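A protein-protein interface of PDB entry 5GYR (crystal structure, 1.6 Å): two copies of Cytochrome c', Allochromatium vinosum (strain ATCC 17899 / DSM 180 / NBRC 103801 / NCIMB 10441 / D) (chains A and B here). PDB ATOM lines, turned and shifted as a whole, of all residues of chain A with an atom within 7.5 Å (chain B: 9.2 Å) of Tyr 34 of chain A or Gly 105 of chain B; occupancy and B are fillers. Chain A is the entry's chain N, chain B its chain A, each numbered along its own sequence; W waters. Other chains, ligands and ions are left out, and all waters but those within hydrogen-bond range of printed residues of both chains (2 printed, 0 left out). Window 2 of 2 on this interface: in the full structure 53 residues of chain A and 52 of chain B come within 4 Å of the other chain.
Water W2 lies within hydrogen-bond range of the backbone carbonyl oxygen (O) of Ala 102 of chain B (2.7 Å), the side-chain hydroxyl (OH) of Tyr 34 of chain A (2.7 Å) and the backbone carbonyl oxygen (O) of Ala 36 of chain A (2.9 Å).
Water W1 lies within hydrogen-bond range of the backbone carbonyl oxygen (O) of Ala 99 of chain B and the backbone carbonyl oxygen (O) of Glu 40 of chain A.
No position is printed for both chains.
Of the 11 pairs that touch across the chains among the printed residues, none has its exchanged pair printed and touching as well.
Among the printed residues, merely in contact across the chains: Ile 26 of chain A with Leu 98 of chain B (3.9 Å), Ile 26 of chain A with Phe 114 of chain B (3.5 Å), Leu 30 of chain A with Ala 107 of chain B (3.6 Å), Leu 30 of chain A with Lys 111 of chain B (3.9 Å), Leu 30 of chain A with Phe 114 of chain B (3.8 Å), Tyr 34 of chain A with Gly 105 of chain B (3.6 Å), Tyr 34 of chain A with Ala 107 of chain B (3.6 Å), Tyr 34 of chain A with Val 110 of chain B (3.4 Å), Val 39 of chain A with Val 110 of chain B (3.9 Å), Glu 40 of chain A with Ala 102 of chain B (3.9 Å) and Glu 40 of chain A with Ala 103 of chain B (3.8 Å).
Asn 29 of chain A touches none of the printed residues of chain B.
No residue of chain B comes within 4 Å of Ala 36 of chain A.
Of the printed residues of chain A, Leu 98 of chain B touches Ile 26 (3.9 Å).
Of the printed residues of chain A, Ala 103 of chain B touches Glu 40.
Ala 109 of chain B touches none of the printed residues of chain A.
The nearest residue of chain B that does not touch Tyr 34 of chain A is Glu 106 of chain B (4.4 Å).
The nearest residue of chain A that does not touch Gly 105 of chain B is Ala 36 of chain A (4.2 Å).
Of the 15 printed residues of chain B, 8 touch a printed residue of chain A.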
ATOM      1  N   ILE A  26      -5.396   7.190 -15.129  1.00  0.00           N
ATOM      2  CA  ILE A  26      -4.676   5.941 -14.880  1.00  0.00           C
ATOM      3  C   ILE A  26      -3.913   6.049 -13.569  1.00  0.00           C
ATOM      4  O   ILE A  26      -3.959   5.142 -12.725  1.00  0.00           O
ATOM      5  CB  ILE A  26      -3.713   5.574 -16.035  1.00  0.00           C
ATOM      6  CG1 ILE A  26      -4.524   5.276 -17.286  1.00  0.00           C
ATOM      7  CG2 ILE A  26      -2.881   4.347 -15.661  1.00  0.00           C
ATOM      8  CD1 ILE A  26      -3.697   5.045 -18.527  1.00  0.00           C
ATOM      9  N   ALA A  28      -4.558   7.939 -11.029  1.00  0.00           N
ATOM     10  CA  ALA A  28      -5.509   7.944  -9.913  1.00  0.00           C
ATOM     11  C   ALA A  28      -5.964   6.525  -9.569  1.00  0.00           C
ATOM     12  O   ALA A  28      -6.078   6.178  -8.391  1.00  0.00           O
ATOM     13  CB  ALA A  28      -6.712   8.815 -10.246  1.00  0.00           C
ATOM     14  N   ASN A  29      -6.232   5.718 -10.597  1.00  0.00           N
ATOM     15  CA  ASN A  29      -6.638   4.320 -10.391  1.00  0.00           C
ATOM     16  C   ASN A  29      -5.549   3.493  -9.738  1.00  0.00           C
ATOM     17  O   ASN A  29      -5.828   2.653  -8.880  1.00  0.00           O
ATOM     18  CB  ASN A  29      -7.058   3.656 -11.703  1.00  0.00           C
ATOM     19  CG  ASN A  29      -8.498   3.932 -12.053  1.00  0.00           C
ATOM     20  OD1 ASN A  29      -9.389   3.163 -11.711  1.00  0.00           O
ATOM     21  ND2 ASN A  29      -8.733   5.027 -12.747  1.00  0.00           N
ATOM     22  N   LEU A  30      -4.308   3.745 -10.136  1.00  0.00           N
ATOM     23  CA  LEU A  30      -3.158   3.045  -9.555  1.00  0.00           C
ATOM     24  C   LEU A  30      -2.910   3.419  -8.093  1.00  0.00           C
ATOM     25  O   LEU A  30      -2.452   2.594  -7.304  1.00  0.00           O
ATOM     26  CB  LEU A  30      -1.888   3.331 -10.361  1.00  0.00           C
ATOM     27  CG  LEU A  30      -1.835   2.730 -11.775  1.00  0.00           C
ATOM     28  CD1 LEU A  30      -0.635   3.261 -12.559  1.00  0.00           C
ATOM     29  CD2 LEU A  30      -1.797   1.209 -11.721  1.00  0.00           C
ATOM     30  N   GLU A  31      -3.197   4.663  -7.736  1.00  0.00           N
ATOM     31  CA  GLU A  31      -2.952   5.142  -6.377  1.00  0.00           C
ATOM     32  C   GLU A  31      -4.160   5.035  -5.439  1.00  0.00           C
ATOM     33  O   GLU A  31      -4.030   5.201  -4.251  1.00  0.00           O
ATOM     34  CB  GLU A  31      -2.465   6.582  -6.426  1.00  0.00           C
ATOM     35  CG  GLU A  31      -1.211   6.755  -7.251  1.00  0.00           C
ATOM     36  CD  GLU A  31      -0.717   8.177  -7.289  1.00  0.00           C
ATOM     37  OE1 GLU A  31      -1.423   9.090  -6.799  1.00  0.00           O
ATOM     38  OE2 GLU A  31       0.393   8.369  -7.812  1.00  0.00           O
ATOM     39  N   GLY A  32      -5.322   4.724  -6.008  1.00  0.00           N
ATOM     40  CA  GLY A  32      -6.541   4.584  -5.214  1.00  0.00           C
ATOM     41  C   GLY A  32      -7.153   3.222  -5.436  1.00  0.00           C
ATOM     42  O   GLY A  32      -6.472   2.200  -5.321  1.00  0.00           O
ATOM     43  N   GLU A  33      -8.439   3.204  -5.756  1.00  0.00           N
ATOM     44  CA  GLU A  33      -9.146   1.956  -5.990  1.00  0.00           C
ATOM     45  C   GLU A  33      -9.230   1.670  -7.480  1.00  0.00           C
ATOM     46  O   GLU A  33      -9.861   2.403  -8.240  1.00  0.00           O
ATOM     47  CB  GLU A  33     -10.530   1.970  -5.348  1.00  0.00           C
ATOM     48  CG  GLU A  33     -10.885   0.621  -4.752  1.00  0.00           C
ATOM     49  CD  GLU A  33     -12.285   0.591  -4.193  1.00  0.00           C
ATOM     50  OE1 GLU A  33     -12.482   1.260  -3.167  1.00  0.00           O
ATOM     51  OE2 GLU A  33     -13.179  -0.076  -4.771  1.00  0.00           O
ATOM     52  N   TYR A  34      -8.582   0.585  -7.876  1.00  0.00           N
ATOM     53  CA  TYR A  34      -8.367   0.281  -9.277  1.00  0.00           C
ATOM     54  C   TYR A  34      -9.650  -0.186  -9.957  1.00  0.00           C
ATOM     55  O   TYR A  34     -10.288  -1.141  -9.515  1.00  0.00           O
ATOM     56  CB  TYR A  34      -7.278  -0.786  -9.392  1.00  0.00           C
ATOM     57  CG  TYR A  34      -6.774  -1.024 -10.789  1.00  0.00           C
ATOM     58  CD1 TYR A  34      -5.685  -0.321 -11.281  1.00  0.00           C
ATOM     59  CD2 TYR A  34      -7.377  -1.969 -11.613  1.00  0.00           C
ATOM     60  CE1 TYR A  34      -5.209  -0.548 -12.561  1.00  0.00           C
ATOM     61  CE2 TYR A  34      -6.912  -2.206 -12.896  1.00  0.00           C
ATOM     62  CZ  TYR A  34      -5.831  -1.489 -13.366  1.00  0.00           C
ATOM     63  OH  TYR A  34      -5.371  -1.712 -14.640  1.00  0.00           O
ATOM     64  N   ASN A  35     -10.016   0.513 -11.024  1.00  0.00           N
ATOM     65  CA  ASN A  35     -11.168   0.168 -11.850  1.00  0.00           C
ATOM     66  C   ASN A  35     -10.609  -0.250 -13.216  1.00  0.00           C
ATOM     67  O   ASN A  35     -10.134   0.586 -13.970  1.00  0.00           O
ATOM     68  CB  ASN A  35     -12.075   1.400 -11.954  1.00  0.00           C
ATOM     69  CG  ASN A  35     -13.306   1.174 -12.812  1.00  0.00           C
ATOM     70  OD1 ASN A  35     -13.299   0.393 -13.760  1.00  0.00           O
ATOM     71  ND2 ASN A  35     -14.364   1.906 -12.504  1.00  0.00           N
ATOM     72  N   ALA A  36     -10.650  -1.553 -13.502  1.00  0.00           N
ATOM     73  CA  ALA A  36      -9.996  -2.119 -14.686  1.00  0.00           C
ATOM     74  C   ALA A  36     -10.555  -1.585 -15.999  1.00  0.00           C
ATOM     75  O   ALA A  36      -9.786  -1.239 -16.886  1.00  0.00           O
ATOM     76  CB  ALA A  36     -10.074  -3.638 -14.664  1.00  0.00           C
ATOM     77  N   ALA A  37     -11.881  -1.500 -16.089  1.00  0.00           N
ATOM     78  CA  ALA A  37     -12.543  -0.980 -17.287  1.00  0.00           C
ATOM     79  C   ALA A  37     -12.177   0.484 -17.531  1.00  0.00           C
ATOM     80  O   ALA A  37     -11.931   0.888 -18.658  1.00  0.00           O
ATOM     81  CB  ALA A  37     -14.048  -1.136 -17.178  1.00  0.00           C
ATOM     82  N   GLN A  38     -12.113   1.264 -16.459  1.00  0.00           N
ATOM     83  CA  GLN A  38     -11.745   2.678 -16.553  1.00  0.00           C
ATOM     84  C   GLN A  38     -10.309   2.857 -17.063  1.00  0.00           C
ATOM     85  O   GLN A  38     -10.039   3.715 -17.901  1.00  0.00           O
ATOM     86  CB  GLN A  38     -11.885   3.356 -15.194  1.00  0.00           C
ATOM     87  CG  GLN A  38     -11.684   4.864 -15.227  1.00  0.00           C
ATOM     88  CD  GLN A  38     -12.113   5.529 -13.938  1.00  0.00           C
ATOM     89  OE1 GLN A  38     -13.177   5.230 -13.401  1.00  0.00           O
ATOM     90  NE2 GLN A  38     -11.297   6.448 -13.440  1.00  0.00           N
ATOM     91  N   VAL A  39      -9.391   2.056 -16.530  1.00  0.00           N
ATOM     92  CA  VAL A  39      -7.991   2.131 -16.943  1.00  0.00           C
ATOM     93  C   VAL A  39      -7.833   1.681 -18.396  1.00  0.00           C
ATOM     94  O   VAL A  39      -7.101   2.292 -19.152  1.00  0.00           O
ATOM     95  CB  VAL A  39      -7.092   1.314 -16.004  1.00  0.00           C
ATOM     96  CG1 VAL A  39      -5.677   1.206 -16.553  1.00  0.00           C
ATOM     97  CG2 VAL A  39      -7.069   1.966 -14.639  1.00  0.00           C
ATOM     98  N   GLU A  40      -8.559   0.627 -18.770  1.00  0.00           N
ATOM     99  CA  GLU A  40      -8.554   0.132 -20.142  1.00  0.00           C
ATOM    100  C   GLU A  40      -9.045   1.225 -21.089  1.00  0.00           C
ATOM    101  O   GLU A  40      -8.434   1.473 -22.122  1.00  0.00           O
ATOM    102  CB  GLU A  40      -9.444  -1.118 -20.265  1.00  0.00           C
ATOM    103  CG  GLU A  40      -9.455  -1.748 -21.655  1.00  0.00           C
ATOM    104  CD  GLU A  40     -10.223  -3.060 -21.740  1.00  0.00           C
ATOM    105  OE1 GLU A  40     -10.385  -3.729 -20.689  1.00  0.00           O
ATOM    106  OE2 GLU A  40     -10.637  -3.416 -22.836  1.00  0.00           O
ATOM    107  N   LEU B  98       0.843  -0.237 -23.314  1.00  0.00           N
ATOM    108  CA  LEU B  98      -0.036   0.142 -22.205  1.00  0.00           C
ATOM    109  C   LEU B  98      -1.479  -0.317 -22.443  1.00  0.00           C
ATOM    110  O   LEU B  98      -2.116  -0.815 -21.536  1.00  0.00           O
ATOM    111  CB  LEU B  98       0.024   1.661 -21.944  1.00  0.00           C
ATOM    112  CG  LEU B  98      -0.928   2.233 -20.882  1.00  0.00           C
ATOM    113  CD1 LEU B  98      -0.712   1.581 -19.518  1.00  0.00           C
ATOM    114  CD2 LEU B  98      -0.753   3.742 -20.781  1.00  0.00           C
ATOM    115  N   ALA B  99      -1.984  -0.158 -23.657  1.00  0.00           N
ATOM    116  CA  ALA B  99      -3.347  -0.590 -23.980  1.00  0.00           C
ATOM    117  C   ALA B  99      -3.490  -2.117 -23.896  1.00  0.00           C
ATOM    118  O   ALA B  99      -4.472  -2.626 -23.367  1.00  0.00           O
ATOM    119  CB  ALA B  99      -3.747  -0.099 -25.364  1.00  0.00           C
ATOM    120  N   GLU B 100      -2.492  -2.838 -24.410  1.00  0.00           N
ATOM    121  CA  GLU B 100      -2.460  -4.297 -24.298  1.00  0.00           C
ATOM    122  C   GLU B 100      -2.486  -4.775 -22.856  1.00  0.00           C
ATOM    123  O   GLU B 100      -3.284  -5.644 -22.478  1.00  0.00           O
ATOM    124  CB  GLU B 100      -1.203  -4.871 -24.974  1.00  0.00           C
ATOM    125  CG  GLU B 100      -1.240  -4.806 -26.478  1.00  0.00           C
ATOM    126  CD  GLU B 100       0.081  -5.207 -27.110  1.00  0.00           C
ATOM    127  OE1 GLU B 100       0.954  -5.759 -26.403  1.00  0.00           O
ATOM    128  OE2 GLU B 100       0.253  -4.960 -28.316  1.00  0.00           O
ATOM    129  N   VAL B 101      -1.602  -4.216 -22.044  1.00  0.00           N
ATOM    130  CA  VAL B 101      -1.495  -4.621 -20.650  1.00  0.00           C
ATOM    131  C   VAL B 101      -2.775  -4.234 -19.892  1.00  0.00           C
ATOM    132  O   VAL B 101      -3.269  -4.984 -19.046  1.00  0.00           O
ATOM    133  CB  VAL B 101      -0.259  -3.974 -19.997  1.00  0.00           C
ATOM    134  CG1 VAL B 101      -0.239  -4.210 -18.504  1.00  0.00           C
ATOM    135  CG2 VAL B 101       1.041  -4.470 -20.641  1.00  0.00           C
ATOM    136  N   ALA B 102      -3.313  -3.057 -20.192  1.00  0.00           N
ATOM    137  CA  ALA B 102      -4.530  -2.595 -19.523  1.00  0.00           C
ATOM    138  C   ALA B 102      -5.709  -3.536 -19.778  1.00  0.00           C
ATOM    139  O   ALA B 102      -6.546  -3.717 -18.907  1.00  0.00           O
ATOM    140  CB  ALA B 102      -4.891  -1.180 -19.956  1.00  0.00           C
ATOM    141  N   ALA B 103      -5.757  -4.133 -20.968  1.00  0.00           N
ATOM    142  CA  ALA B 103      -6.833  -5.070 -21.306  1.00  0.00           C
ATOM    143  C   ALA B 103      -6.809  -6.333 -20.440  1.00  0.00           C
ATOM    144  O   ALA B 103      -7.822  -7.003 -20.296  1.00  0.00           O
ATOM    145  CB  ALA B 103      -6.780  -5.436 -22.779  1.00  0.00           C
ATOM    146  N   THR B 104      -5.652  -6.655 -19.864  1.00  0.00           N
ATOM    147  CA  THR B 104      -5.535  -7.823 -18.971  1.00  0.00           C
ATOM    148  C   THR B 104      -6.086  -7.571 -17.560  1.00  0.00           C
ATOM    149  O   THR B 104      -6.366  -8.508 -16.820  1.00  0.00           O
ATOM    150  CB  THR B 104      -4.071  -8.308 -18.831  1.00  0.00           C
ATOM    151  OG1 THR B 104      -3.321  -7.401 -18.010  1.00  0.00           O
ATOM    152  CG2 THR B 104      -3.409  -8.476 -20.197  1.00  0.00           C
ATOM    153  N   GLY B 105      -6.180  -6.295 -17.194  1.00  0.00           N
ATOM    154  CA  GLY B 105      -6.707  -5.896 -15.897  1.00  0.00           C
ATOM    155  C   GLY B 105      -5.688  -5.942 -14.772  1.00  0.00           C
ATOM    156  O   GLY B 105      -6.026  -5.649 -13.626  1.00  0.00           O
ATOM    157  N   GLU B 106      -4.434  -6.275 -15.093  1.00  0.00           N
ATOM    158  CA  GLU B 106      -3.408  -6.466 -14.060  1.00  0.00           C
ATOM    159  C   GLU B 106      -2.734  -5.143 -13.686  1.00  0.00           C
ATOM    160  O   GLU B 106      -1.887  -4.652 -14.410  1.00  0.00           O
ATOM    161  CB  GLU B 106      -2.327  -7.470 -14.507  1.00  0.00           C
ATOM    162  CG  GLU B 106      -1.469  -8.030 -13.354  1.00  0.00           C
ATOM    163  CD  GLU B 106      -0.228  -8.798 -13.821  1.00  0.00           C
ATOM    164  OE1 GLU B 106       0.444  -9.479 -13.007  1.00  0.00           O
ATOM    165  OE2 GLU B 106       0.073  -8.763 -15.020  1.00  0.00           O
ATOM    166  N   ALA B 107      -3.095  -4.612 -12.514  1.00  0.00           N
ATOM    167  CA  ALA B 107      -2.629  -3.285 -12.093  1.00  0.00           C
ATOM    168  C   ALA B 107      -1.110  -3.144 -12.015  1.00  0.00           C
ATOM    169  O   ALA B 107      -0.569  -2.096 -12.365  1.00  0.00           O
ATOM    170  CB  ALA B 107      -3.251  -2.914 -10.756  1.00  0.00           C
ATOM    171  N   GLU B 108      -0.410  -4.174 -11.546  1.00  0.00           N
ATOM    172  CA  GLU B 108       1.040  -4.047 -11.401  1.00  0.00           C
ATOM    173  C   GLU B 108       1.746  -3.963 -12.756  1.00  0.00           C
ATOM    174  O   GLU B 108       2.709  -3.221 -12.903  1.00  0.00           O
ATOM    175  CB  GLU B 108       1.636  -5.175 -10.555  1.00  0.00           C
ATOM    176  CG  GLU B 108       2.906  -4.806  -9.790  1.00  0.00           C
ATOM    177  CD  GLU B 108       2.740  -3.563  -8.906  1.00  0.00           C
ATOM    178  OE1 GLU B 108       1.636  -2.963  -8.871  1.00  0.00           O
ATOM    179  OE2 GLU B 108       3.727  -3.175  -8.243  1.00  0.00           O
ATOM    180  N   ALA B 109       1.257  -4.714 -13.740  1.00  0.00           N
ATOM    181  CA  ALA B 109       1.799  -4.645 -15.093  1.00  0.00           C
ATOM    182  C   ALA B 109       1.470  -3.288 -15.726  1.00  0.00           C
ATOM    183  O   ALA B 109       2.303  -2.685 -16.401  1.00  0.00           O
ATOM    184  CB  ALA B 109       1.258  -5.783 -15.942  1.00  0.00           C
ATOM    185  N   VAL B 110       0.258  -2.809 -15.491  1.00  0.00           N
ATOM    186  CA  VAL B 110      -0.156  -1.483 -15.969  1.00  0.00           C
ATOM    187  C   VAL B 110       0.749  -0.397 -15.393  1.00  0.00           C
ATOM    188  O   VAL B 110       1.164   0.511 -16.107  1.00  0.00           O
ATOM    189  CB  VAL B 110      -1.630  -1.180 -15.628  1.00  0.00           C
ATOM    190  CG1 VAL B 110      -1.958   0.293 -15.857  1.00  0.00           C
ATOM    191  CG2 VAL B 110      -2.542  -2.050 -16.473  1.00  0.00           C
ATOM    192  N   LYS B 111       1.075  -0.503 -14.107  1.00  0.00           N
ATOM    193  CA  LYS B 111       1.925   0.492 -13.464  1.00  0.00           C
ATOM    194  C   LYS B 111       3.248   0.635 -14.215  1.00  0.00           C
ATOM    195  O   LYS B 111       3.712   1.746 -14.471  1.00  0.00           O
ATOM    196  CB  LYS B 111       2.171   0.148 -11.985  1.00  0.00           C
ATOM    197  CG  LYS B 111       3.015   1.176 -11.271  1.00  0.00           C
ATOM    198  CD  LYS B 111       3.148   0.920  -9.773  1.00  0.00           C
ATOM    199  CE  LYS B 111       4.431   1.533  -9.211  1.00  0.00           C
ATOM    200  NZ  LYS B 111       4.272   1.986  -7.800  1.00  0.00           N
ATOM    201  N   PHE B 114       2.549   2.084 -17.737  1.00  0.00           N
ATOM    202  CA  PHE B 114       2.206   3.486 -17.561  1.00  0.00           C
ATOM    203  C   PHE B 114       3.459   4.345 -17.401  1.00  0.00           C
ATOM    204  O   PHE B 114       3.559   5.434 -17.966  1.00  0.00           O
ATOM    205  CB  PHE B 114       1.295   3.616 -16.340  1.00  0.00           C
ATOM    206  CG  PHE B 114       0.915   5.022 -16.010  1.00  0.00           C
ATOM    207  CD1 PHE B 114       0.124   5.762 -16.873  1.00  0.00           C
ATOM    208  CD2 PHE B 114       1.341   5.603 -14.827  1.00  0.00           C
ATOM    209  CE1 PHE B 114      -0.230   7.062 -16.561  1.00  0.00           C
ATOM    210  CE2 PHE B 114       0.990   6.901 -14.512  1.00  0.00           C
ATOM    211  CZ  PHE B 114       0.209   7.632 -15.388  1.00  0.00           C
HETATM  212  O   HOH W   1      -6.540  -0.792 -23.073  1.00  0.00           O
HETATM  213  O   HOH W   2      -7.135  -2.422 -16.591  1.00  0.00           O
